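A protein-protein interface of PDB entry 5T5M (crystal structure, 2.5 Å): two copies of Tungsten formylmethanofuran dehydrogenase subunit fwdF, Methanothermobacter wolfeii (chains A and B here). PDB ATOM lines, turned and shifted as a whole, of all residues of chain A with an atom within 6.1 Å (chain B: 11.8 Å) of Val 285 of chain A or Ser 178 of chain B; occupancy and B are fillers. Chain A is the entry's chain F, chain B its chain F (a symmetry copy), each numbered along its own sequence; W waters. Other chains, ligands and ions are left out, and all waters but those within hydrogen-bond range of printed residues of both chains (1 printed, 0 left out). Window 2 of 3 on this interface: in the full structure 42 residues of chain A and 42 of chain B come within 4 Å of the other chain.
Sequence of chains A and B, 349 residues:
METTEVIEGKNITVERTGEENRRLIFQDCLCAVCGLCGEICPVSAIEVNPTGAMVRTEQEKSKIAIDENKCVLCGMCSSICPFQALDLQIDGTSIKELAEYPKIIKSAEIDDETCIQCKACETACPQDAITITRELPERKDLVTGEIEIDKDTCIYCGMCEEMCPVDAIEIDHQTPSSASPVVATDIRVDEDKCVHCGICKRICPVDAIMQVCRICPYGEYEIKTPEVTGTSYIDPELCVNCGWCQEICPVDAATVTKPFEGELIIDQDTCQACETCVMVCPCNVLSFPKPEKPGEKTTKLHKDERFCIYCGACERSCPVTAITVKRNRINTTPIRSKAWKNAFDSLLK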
ATOM      1  N   TRP A 244      -8.303 -12.015  20.052  1.00  0.00           N
ATOM      2  CA  TRP A 244      -7.675 -12.157  18.737  1.00  0.00           C
ATOM      3  C   TRP A 244      -6.679 -13.312  18.720  1.00  0.00           C
ATOM      4  O   TRP A 244      -6.584 -14.053  17.733  1.00  0.00           O
ATOM      5  CB  TRP A 244      -6.960 -10.862  18.341  1.00  0.00           C
ATOM      6  CG  TRP A 244      -7.748  -9.963  17.455  1.00  0.00           C
ATOM      7  CD1 TRP A 244      -8.360  -8.810  17.810  1.00  0.00           C
ATOM      8  CD2 TRP A 244      -7.999 -10.137  16.054  1.00  0.00           C
ATOM      9  NE1 TRP A 244      -8.980  -8.251  16.727  1.00  0.00           N
ATOM     10  CE2 TRP A 244      -8.774  -9.047  15.636  1.00  0.00           C
ATOM     11  CE3 TRP A 244      -7.636 -11.104  15.116  1.00  0.00           C
ATOM     12  CZ2 TRP A 244      -9.197  -8.898  14.327  1.00  0.00           C
ATOM     13  CZ3 TRP A 244      -8.061 -10.955  13.822  1.00  0.00           C
ATOM     14  CH2 TRP A 244      -8.834  -9.866  13.437  1.00  0.00           C
ATOM     15  N   LEU A 264     -23.302  -5.467  20.012  1.00  0.00           N
ATOM     16  CA  LEU A 264     -22.966  -4.308  19.191  1.00  0.00           C
ATOM     17  C   LEU A 264     -24.043  -4.100  18.141  1.00  0.00           C
ATOM     18  O   LEU A 264     -24.410  -5.047  17.440  1.00  0.00           O
ATOM     19  CB  LEU A 264     -21.629  -4.516  18.479  1.00  0.00           C
ATOM     20  CG  LEU A 264     -20.349  -4.028  19.128  1.00  0.00           C
ATOM     21  CD1 LEU A 264     -19.206  -4.151  18.109  1.00  0.00           C
ATOM     22  CD2 LEU A 264     -20.502  -2.594  19.625  1.00  0.00           C
ATOM     23  N   CYS A 281     -11.186   1.824  18.643  1.00  0.00           N
ATOM     24  CA  CYS A 281     -11.432   0.506  19.204  1.00  0.00           C
ATOM     25  C   CYS A 281     -10.126  -0.157  19.633  1.00  0.00           C
ATOM     26  O   CYS A 281      -9.267  -0.424  18.777  1.00  0.00           O
ATOM     27  CB  CYS A 281     -12.163  -0.364  18.184  1.00  0.00           C
ATOM     28  SG  CYS A 281     -12.272  -2.098  18.668  1.00  0.00           S
ATOM     29  N   PRO A 282      -9.932  -0.438  20.923  1.00  0.00           N
ATOM     30  CA  PRO A 282      -8.694  -1.084  21.376  1.00  0.00           C
ATOM     31  C   PRO A 282      -8.627  -2.570  21.084  1.00  0.00           C
ATOM     32  O   PRO A 282      -7.615  -3.202  21.407  1.00  0.00           O
ATOM     33  CB  PRO A 282      -8.714  -0.839  22.886  1.00  0.00           C
ATOM     34  CG  PRO A 282     -10.148  -0.763  23.223  1.00  0.00           C
ATOM     35  CD  PRO A 282     -10.862  -0.183  22.033  1.00  0.00           C
ATOM     36  N   CYS A 283      -9.664  -3.137  20.480  1.00  0.00           N
ATOM     37  CA  CYS A 283      -9.728  -4.566  20.232  1.00  0.00           C
ATOM     38  C   CYS A 283      -9.761  -4.913  18.753  1.00  0.00           C
ATOM     39  O   CYS A 283      -9.874  -6.097  18.413  1.00  0.00           O
ATOM     40  CB  CYS A 283     -10.962  -5.154  20.932  1.00  0.00           C
ATOM     41  SG  CYS A 283     -10.809  -5.172  22.736  1.00  0.00           S
ATOM     42  N   ASN A 284      -9.684  -3.925  17.868  1.00  0.00           N
ATOM     43  CA  ASN A 284      -9.690  -4.184  16.433  1.00  0.00           C
ATOM     44  C   ASN A 284     -10.965  -4.897  15.989  1.00  0.00           C
ATOM     45  O   ASN A 284     -10.932  -5.817  15.172  1.00  0.00           O
ATOM     46  CB  ASN A 284      -8.456  -4.988  16.036  1.00  0.00           C
ATOM     47  CG  ASN A 284      -7.575  -4.238  15.118  1.00  0.00           C
ATOM     48  OD1 ASN A 284      -7.777  -4.255  13.899  1.00  0.00           O
ATOM     49  ND2 ASN A 284      -6.586  -3.551  15.683  1.00  0.00           N
ATOM     50  N   VAL A 285     -12.107  -4.455  16.515  1.00  0.00           N
ATOM     51  CA  VAL A 285     -13.376  -5.057  16.131  1.00  0.00           C
ATOM     52  C   VAL A 285     -13.861  -4.494  14.801  1.00  0.00           C
ATOM     53  O   VAL A 285     -14.424  -5.223  13.979  1.00  0.00           O
ATOM     54  CB  VAL A 285     -14.420  -4.844  17.249  1.00  0.00           C
ATOM     55  CG1 VAL A 285     -15.760  -5.466  16.865  1.00  0.00           C
ATOM     56  CG2 VAL A 285     -13.929  -5.422  18.572  1.00  0.00           C
ATOM     57  N   LEU A 286     -13.639  -3.203  14.563  1.00  0.00           N
ATOM     58  CA  LEU A 286     -14.320  -2.459  13.509  1.00  0.00           C
ATOM     59  C   LEU A 286     -13.364  -2.131  12.366  1.00  0.00           C
ATOM     60  O   LEU A 286     -12.190  -1.835  12.596  1.00  0.00           O
ATOM     61  CB  LEU A 286     -14.920  -1.174  14.084  1.00  0.00           C
ATOM     62  CG  LEU A 286     -15.870  -1.413  15.267  1.00  0.00           C
ATOM     63  CD1 LEU A 286     -16.110  -0.148  16.079  1.00  0.00           C
ATOM     64  CD2 LEU A 286     -17.193  -1.997  14.792  1.00  0.00           C
ATOM     65  N   SER A 287     -13.870  -2.174  11.132  1.00  0.00           N
ATOM     66  CA  SER A 287     -13.019  -2.011   9.958  1.00  0.00           C
ATOM     67  C   SER A 287     -13.860  -1.643   8.742  1.00  0.00           C
ATOM     68  O   SER A 287     -15.085  -1.781   8.736  1.00  0.00           O
ATOM     69  CB  SER A 287     -12.225  -3.289   9.661  1.00  0.00           C
ATOM     70  OG  SER A 287     -13.110  -4.325   9.286  1.00  0.00           O
ATOM     71  N   HIS A 302     -17.903  -2.625   9.276  1.00  0.00           N
ATOM     72  CA  HIS A 302     -17.906  -4.050   9.560  1.00  0.00           C
ATOM     73  C   HIS A 302     -17.383  -4.303  10.968  1.00  0.00           C
ATOM     74  O   HIS A 302     -16.460  -3.626  11.431  1.00  0.00           O
ATOM     75  CB  HIS A 302     -17.049  -4.816   8.548  1.00  0.00           C
ATOM     76  CG  HIS A 302     -17.052  -6.296   8.763  1.00  0.00           C
ATOM     77  ND1 HIS A 302     -15.998  -6.966   9.353  1.00  0.00           N
ATOM     78  CD2 HIS A 302     -17.992  -7.233   8.495  1.00  0.00           C
ATOM     79  CE1 HIS A 302     -16.283  -8.253   9.420  1.00  0.00           C
ATOM     80  NE2 HIS A 302     -17.487  -8.441   8.909  1.00  0.00           N
ATOM     81  N   LYS A 303     -17.972  -5.291  11.635  1.00  0.00           N
ATOM     82  CA  LYS A 303     -17.605  -5.669  12.988  1.00  0.00           C
ATOM     83  C   LYS A 303     -17.427  -7.177  13.076  1.00  0.00           C
ATOM     84  O   LYS A 303     -18.022  -7.932  12.303  1.00  0.00           O
ATOM     85  CB  LYS A 303     -18.685  -5.237  13.982  1.00  0.00           C
ATOM     86  CG  LYS A 303     -20.060  -5.749  13.588  1.00  0.00           C
ATOM     87  CD  LYS A 303     -21.040  -5.726  14.735  1.00  0.00           C
ATOM     88  CE  LYS A 303     -22.270  -6.520  14.379  1.00  0.00           C
ATOM     89  NZ  LYS A 303     -23.093  -6.737  15.581  1.00  0.00           N
ATOM     90  N   ASP A 304     -16.613  -7.610  14.038  1.00  0.00           N
ATOM     91  CA  ASP A 304     -16.514  -9.019  14.422  1.00  0.00           C
ATOM     92  C   ASP A 304     -16.553  -9.072  15.951  1.00  0.00           C
ATOM     93  O   ASP A 304     -15.536  -8.834  16.612  1.00  0.00           O
ATOM     94  CB  ASP A 304     -15.244  -9.655  13.859  1.00  0.00           C
ATOM     95  CG  ASP A 304     -15.313 -11.178  13.817  1.00  0.00           C
ATOM     96  OD1 ASP A 304     -15.807 -11.785  14.789  1.00  0.00           O
ATOM     97  OD2 ASP A 304     -14.867 -11.776  12.815  1.00  0.00           O
ATOM     98  N   GLU A 305     -17.726  -9.371  16.521  1.00  0.00           N
ATOM     99  CA  GLU A 305     -17.873  -9.308  17.972  1.00  0.00           C
ATOM    100  C   GLU A 305     -17.020 -10.339  18.694  1.00  0.00           C
ATOM    101  O   GLU A 305     -16.842 -10.216  19.910  1.00  0.00           O
ATOM    102  CB  GLU A 305     -19.349  -9.474  18.385  1.00  0.00           C
ATOM    103  CG  GLU A 305     -20.213  -8.256  18.063  1.00  0.00           C
ATOM    104  CD  GLU A 305     -21.601  -8.291  18.700  1.00  0.00           C
ATOM    105  OE1 GLU A 305     -21.730  -8.704  19.871  1.00  0.00           O
ATOM    106  OE2 GLU A 305     -22.571  -7.896  18.024  1.00  0.00           O
ATOM    107  N   ARG A 306     -16.474 -11.333  17.983  1.00  0.00           N
ATOM    108  CA  ARG A 306     -15.519 -12.253  18.601  1.00  0.00           C
ATOM    109  C   ARG A 306     -14.407 -11.517  19.336  1.00  0.00           C
ATOM    110  O   ARG A 306     -13.832 -12.057  20.287  1.00  0.00           O
ATOM    111  CB  ARG A 306     -14.895 -13.169  17.550  1.00  0.00           C
ATOM    112  CG  ARG A 306     -15.821 -14.234  17.019  1.00  0.00           C
ATOM    113  CD  ARG A 306     -15.102 -15.150  16.045  1.00  0.00           C
ATOM    114  NE  ARG A 306     -14.576 -14.421  14.898  1.00  0.00           N
ATOM    115  CZ  ARG A 306     -13.672 -14.908  14.049  1.00  0.00           C
ATOM    116  NH1 ARG A 306     -13.170 -16.124  14.217  1.00  0.00           N
ATOM    117  NH2 ARG A 306     -13.253 -14.172  13.033  1.00  0.00           N
ATOM    118  N   PHE A 307     -14.082 -10.296  18.908  1.00  0.00           N
ATOM    119  CA  PHE A 307     -12.986  -9.528  19.486  1.00  0.00           C
ATOM    120  C   PHE A 307     -13.454  -8.402  20.393  1.00  0.00           C
ATOM    121  O   PHE A 307     -12.622  -7.756  21.036  1.00  0.00           O
ATOM    122  CB  PHE A 307     -12.106  -8.965  18.356  1.00  0.00           C
ATOM    123  CG  PHE A 307     -11.795  -9.989  17.304  1.00  0.00           C
ATOM    124  CD1 PHE A 307     -11.279 -11.225  17.665  1.00  0.00           C
ATOM    125  CD2 PHE A 307     -12.081  -9.753  15.970  1.00  0.00           C
ATOM    126  CE1 PHE A 307     -11.019 -12.196  16.713  1.00  0.00           C
ATOM    127  CE2 PHE A 307     -11.827 -10.719  15.015  1.00  0.00           C
ATOM    128  CZ  PHE A 307     -11.292 -11.946  15.390  1.00  0.00           C
ATOM    129  N   CYS A 308     -14.760  -8.187  20.495  1.00  0.00           N
ATOM    130  CA  CYS A 308     -15.307  -7.090  21.270  1.00  0.00           C
ATOM    131  C   CYS A 308     -15.382  -7.450  22.750  1.00  0.00           C
ATOM    132  O   CYS A 308     -15.697  -8.585  23.115  1.00  0.00           O
ATOM    133  CB  CYS A 308     -16.688  -6.753  20.725  1.00  0.00           C
ATOM    134  SG  CYS A 308     -17.578  -5.530  21.664  1.00  0.00           S
ATOM    135  N   ILE A 309     -15.075  -6.472  23.606  1.00  0.00           N
ATOM    136  CA  ILE A 309     -15.183  -6.620  25.056  1.00  0.00           C
ATOM    137  C   ILE A 309     -16.285  -5.753  25.648  1.00  0.00           C
ATOM    138  O   ILE A 309     -16.476  -5.762  26.874  1.00  0.00           O
ATOM    139  CB  ILE A 309     -13.841  -6.320  25.749  1.00  0.00           C
ATOM    140  CG1 ILE A 309     -13.416  -4.867  25.500  1.00  0.00           C
ATOM    141  CG2 ILE A 309     -12.767  -7.305  25.261  1.00  0.00           C
ATOM    142  CD1 ILE A 309     -12.298  -4.390  26.387  1.00  0.00           C
ATOM    143  N   GLN B 174       0.772  -8.593   6.798  1.00  0.00           N
ATOM    144  CA  GLN B 174      -0.188  -7.519   7.036  1.00  0.00           C
ATOM    145  C   GLN B 174      -0.613  -7.543   8.497  1.00  0.00           C
ATOM    146  O   GLN B 174      -0.469  -8.554   9.191  1.00  0.00           O
ATOM    147  CB  GLN B 174      -1.419  -7.646   6.134  1.00  0.00           C
ATOM    148  CG  GLN B 174      -2.384  -8.752   6.536  1.00  0.00           C
ATOM    149  CD  GLN B 174      -3.704  -8.648   5.813  1.00  0.00           C
ATOM    150  OE1 GLN B 174      -3.822  -7.935   4.821  1.00  0.00           O
ATOM    151  NE2 GLN B 174      -4.712  -9.347   6.317  1.00  0.00           N
ATOM    152  N   THR B 175      -1.151  -6.408   8.951  1.00  0.00           N
ATOM    153  CA  THR B 175      -1.857  -6.380  10.228  1.00  0.00           C
ATOM    154  C   THR B 175      -3.298  -6.823  10.010  1.00  0.00           C
ATOM    155  O   THR B 175      -3.970  -6.293   9.121  1.00  0.00           O
ATOM    156  CB  THR B 175      -1.839  -4.989  10.852  1.00  0.00           C
ATOM    157  OG1 THR B 175      -0.483  -4.578  11.058  1.00  0.00           O
ATOM    158  CG2 THR B 175      -2.566  -4.996  12.202  1.00  0.00           C
ATOM    159  N   PRO B 176      -3.801  -7.788  10.777  1.00  0.00           N
ATOM    160  CA  PRO B 176      -5.189  -8.220  10.590  1.00  0.00           C
ATOM    161  C   PRO B 176      -6.193  -7.109  10.875  1.00  0.00           C
ATOM    162  O   PRO B 176      -5.913  -6.116  11.555  1.00  0.00           O
ATOM    163  CB  PRO B 176      -5.344  -9.379  11.586  1.00  0.00           C
ATOM    164  CG  PRO B 176      -3.955  -9.825  11.877  1.00  0.00           C
ATOM    165  CD  PRO B 176      -3.097  -8.609  11.772  1.00  0.00           C
ATOM    166  N   SER B 177      -7.374  -7.289  10.305  1.00  0.00           N
ATOM    167  CA  SER B 177      -8.540  -6.484  10.601  1.00  0.00           C
ATOM    168  C   SER B 177      -9.717  -7.437  10.696  1.00  0.00           C
ATOM    169  O   SER B 177      -9.640  -8.590  10.256  1.00  0.00           O
ATOM    170  CB  SER B 177      -8.793  -5.422   9.520  1.00  0.00           C
ATOM    171  OG  SER B 177      -9.363  -6.019   8.366  1.00  0.00           O
ATOM    172  N   SER B 178     -10.813  -6.967  11.283  1.00  0.00           N
ATOM    173  CA  SER B 178     -11.984  -7.828  11.349  1.00  0.00           C
ATOM    174  C   SER B 178     -12.469  -8.190   9.953  1.00  0.00           C
ATOM    175  O   SER B 178     -13.108  -9.236   9.779  1.00  0.00           O
ATOM    176  CB  SER B 178     -13.101  -7.162  12.162  1.00  0.00           C
ATOM    177  OG  SER B 178     -13.515  -5.931  11.598  1.00  0.00           O
ATOM    178  N   ALA B 179     -12.142  -7.365   8.957  1.00  0.00           N
ATOM    179  CA  ALA B 179     -12.527  -7.611   7.577  1.00  0.00           C
ATOM    180  C   ALA B 179     -11.550  -8.521   6.860  1.00  0.00           C
ATOM    181  O   ALA B 179     -11.895  -9.084   5.815  1.00  0.00           O
ATOM    182  CB  ALA B 179     -12.628  -6.283   6.815  1.00  0.00           C
ATOM    183  N   SER B 180     -10.338  -8.661   7.391  1.00  0.00           N
ATOM    184  CA  SER B 180      -9.301  -9.488   6.782  1.00  0.00           C
ATOM    185  C   SER B 180      -8.506 -10.121   7.913  1.00  0.00           C
ATOM    186  O   SER B 180      -7.388  -9.700   8.223  1.00  0.00           O
ATOM    187  CB  SER B 180      -8.409  -8.648   5.868  1.00  0.00           C
ATOM    188  OG  SER B 180      -7.419  -9.437   5.219  1.00  0.00           O
ATOM    189  N   PRO B 181      -9.090 -11.137   8.595  1.00  0.00           N
ATOM    190  CA  PRO B 181      -8.527 -11.693   9.835  1.00  0.00           C
ATOM    191  C   PRO B 181      -7.368 -12.666   9.630  1.00  0.00           C
ATOM    192  O   PRO B 181      -7.377 -13.790  10.136  1.00  0.00           O
ATOM    193  CB  PRO B 181      -9.735 -12.392  10.463  1.00  0.00           C
ATOM    194  CG  PRO B 181     -10.540 -12.799   9.301  1.00  0.00           C
ATOM    195  CD  PRO B 181     -10.414 -11.709   8.301  1.00  0.00           C
ATOM    196  N   VAL B 182      -6.346 -12.220   8.907  1.00  0.00           N
ATOM    197  CA  VAL B 182      -5.204 -13.059   8.569  1.00  0.00           C
ATOM    198  C   VAL B 182      -3.927 -12.236   8.689  1.00  0.00           C
ATOM    199  O   VAL B 182      -3.918 -11.029   8.431  1.00  0.00           O
ATOM    200  CB  VAL B 182      -5.360 -13.654   7.148  1.00  0.00           C
ATOM    201  CG1 VAL B 182      -6.537 -14.652   7.111  1.00  0.00           C
ATOM    202  CG2 VAL B 182      -5.568 -12.557   6.114  1.00  0.00           C
ATOM    203  N   VAL B 183      -2.836 -12.898   9.096  1.00  0.00           N
ATOM    204  CA  VAL B 183      -1.552 -12.216   9.229  1.00  0.00           C
ATOM    205  C   VAL B 183      -0.765 -12.166   7.920  1.00  0.00           C
ATOM    206  O   VAL B 183       0.349 -11.623   7.898  1.00  0.00           O
ATOM    207  CB  VAL B 183      -0.674 -12.870  10.320  1.00  0.00           C
ATOM    208  CG1 VAL B 183      -1.415 -12.884  11.657  1.00  0.00           C
ATOM    209  CG2 VAL B 183      -0.228 -14.279   9.914  1.00  0.00           C
HETATM  210  O   HOH W   1     -10.405  -4.332  12.752  1.00  0.00           O
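No position is printed for both chains. Of the 12 pairs that touch across the chains among the printed residues, none has its exchanged pair printed and touching as well.
Trp 244 of chain A touches Pro 176 of chain B (CZ3 to CB, 3.9 Å). Trp 244 of chain A touches Ser 177 of chain B. Ser 178 of chain B touches Trp 244 of chain A (N to CZ2, 3.95 Å). Asn 284 of chain A touches Pro 176 of chain B. O of Asn 284 of chain A touches CB of Ser 178 of chain B (3.9 Å). Leu 286 of chain A touches Ser 178 of chain B (C to OG, 3.9 Å). His 302 of chain A touches Ser 178 of chain B (CE1 to O, 3.3 Å). His 302 of chain A touches Ala 179 of chain B (ND1 to N, 3.9 Å). Ser 178 of chain B touches Asp 304 of chain A (CB to CB, 3.7 Å).
The backbone NH of Ala 179 of chain B sits close to the side-chain hydroxyl of Ser 287 of chain A (3.2 Å). The backbone carbonyl oxygen (O) of Val 285 of chain A lies within hydrogen-bond range of the side-chain hydroxyl (OG) of Ser 178 of chain B (2.6 Å). OG of Ser 287 of chain A is in hydrogen-bond range of OG of Ser 178 of chain B, at 2.8 Å.
Water W1 lies within hydrogen-bond range of OD1 of Asn 284 of chain A, N of Ser 178 of chain B and O of Leu 286 of chain A.
Val 285 of chain A touches one residue of chain B. Of chain A, only Trp 244, Asn 284, Val 285, Leu 286, Ser 287, His 302 and Asp 304 come within 4 Å of Ser 178 of chain B. No residue of chain B comes within 4 Å of Cys 281 of chain A. Of chain B, only Pro 176 (3.5 Å) and Ser 178 (3.9 Å) come within 4 Å of Asn 284 of chain A. Leu 286 of chain A touches one residue of chain B. Printed residues of chain B within 4 Å of Ser 287 of chain A: Ser 178 and Ala 179. Of chain B, only Ser 178 (3.3 Å) and Ala 179 (3.9 Å) come within 4 Å of His 302 of chain A. No residue of chain B comes within 4 Å of Lys 303 of chain A. No residue of chain B comes within 4 Å of Phe 307 of chain A. Of the printed residues of chain B, Trp 244 of chain A touches Pro 176, Ser 177 and Ser 178. Printed residues of chain A within 4 Å of Ala 179 of chain B: Ser 287 and His 302. Of the printed residues of chain A, Pro 176 of chain B touches Trp 244 and Asn 284. Gln 174 of chain B touches none of the printed residues of chain A. Thr 175 of chain B touches none of the printed residues of chain A. The nearest residue of chain A that does not touch Ser 178 of chain B is Lys 303 of chain A (4.3 Å).
O of Cys 283 of chain A sits at hydrogen-bond distance from NE1 of Trp 244 of chain A (2.9 Å). N of Ala 179 of chain B lies close to OG of Ser 177 of chain B, 3.1 Å away. The guanidinium group (NH2) of Arg 306 of chain A is in salt-bridge range of the side-chain carboxylate (OD2) of Asp 304 of chain A. SG of Cys 281 of chain A sits close to N of Val 285 of chain A (3.2 Å). The side-chain hydroxyl of Ser 177 of chain B lies within hydrogen-bond range of the backbone NH of Ser 180 of chain B (3.0 Å). The backbone carbonyl oxygen (O) of Val 285 of chain A sits at hydrogen-bond distance from the backbone NH (N) of Asp 304 of chain A.
Hydrophobic or aromatic side chains of chain A that line the printed part of chain B: Trp 244 and His 302. Of the 10 printed residues of chain B, 4 touch a printed residue of chain A. Printed residues of chain B that touch a printed residue of chain A: Pro 176, Ser 177, Ser 178 and Ala 179. Hydrophobic or aromatic side chains of chain B within 4 Å of the printed part of chain A: Pro 176 and Ala 179. Among the printed residues, no Asp or Glu carboxylate lies within 4 Å of a Lys or Arg side-chain nitrogen of the other chain.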
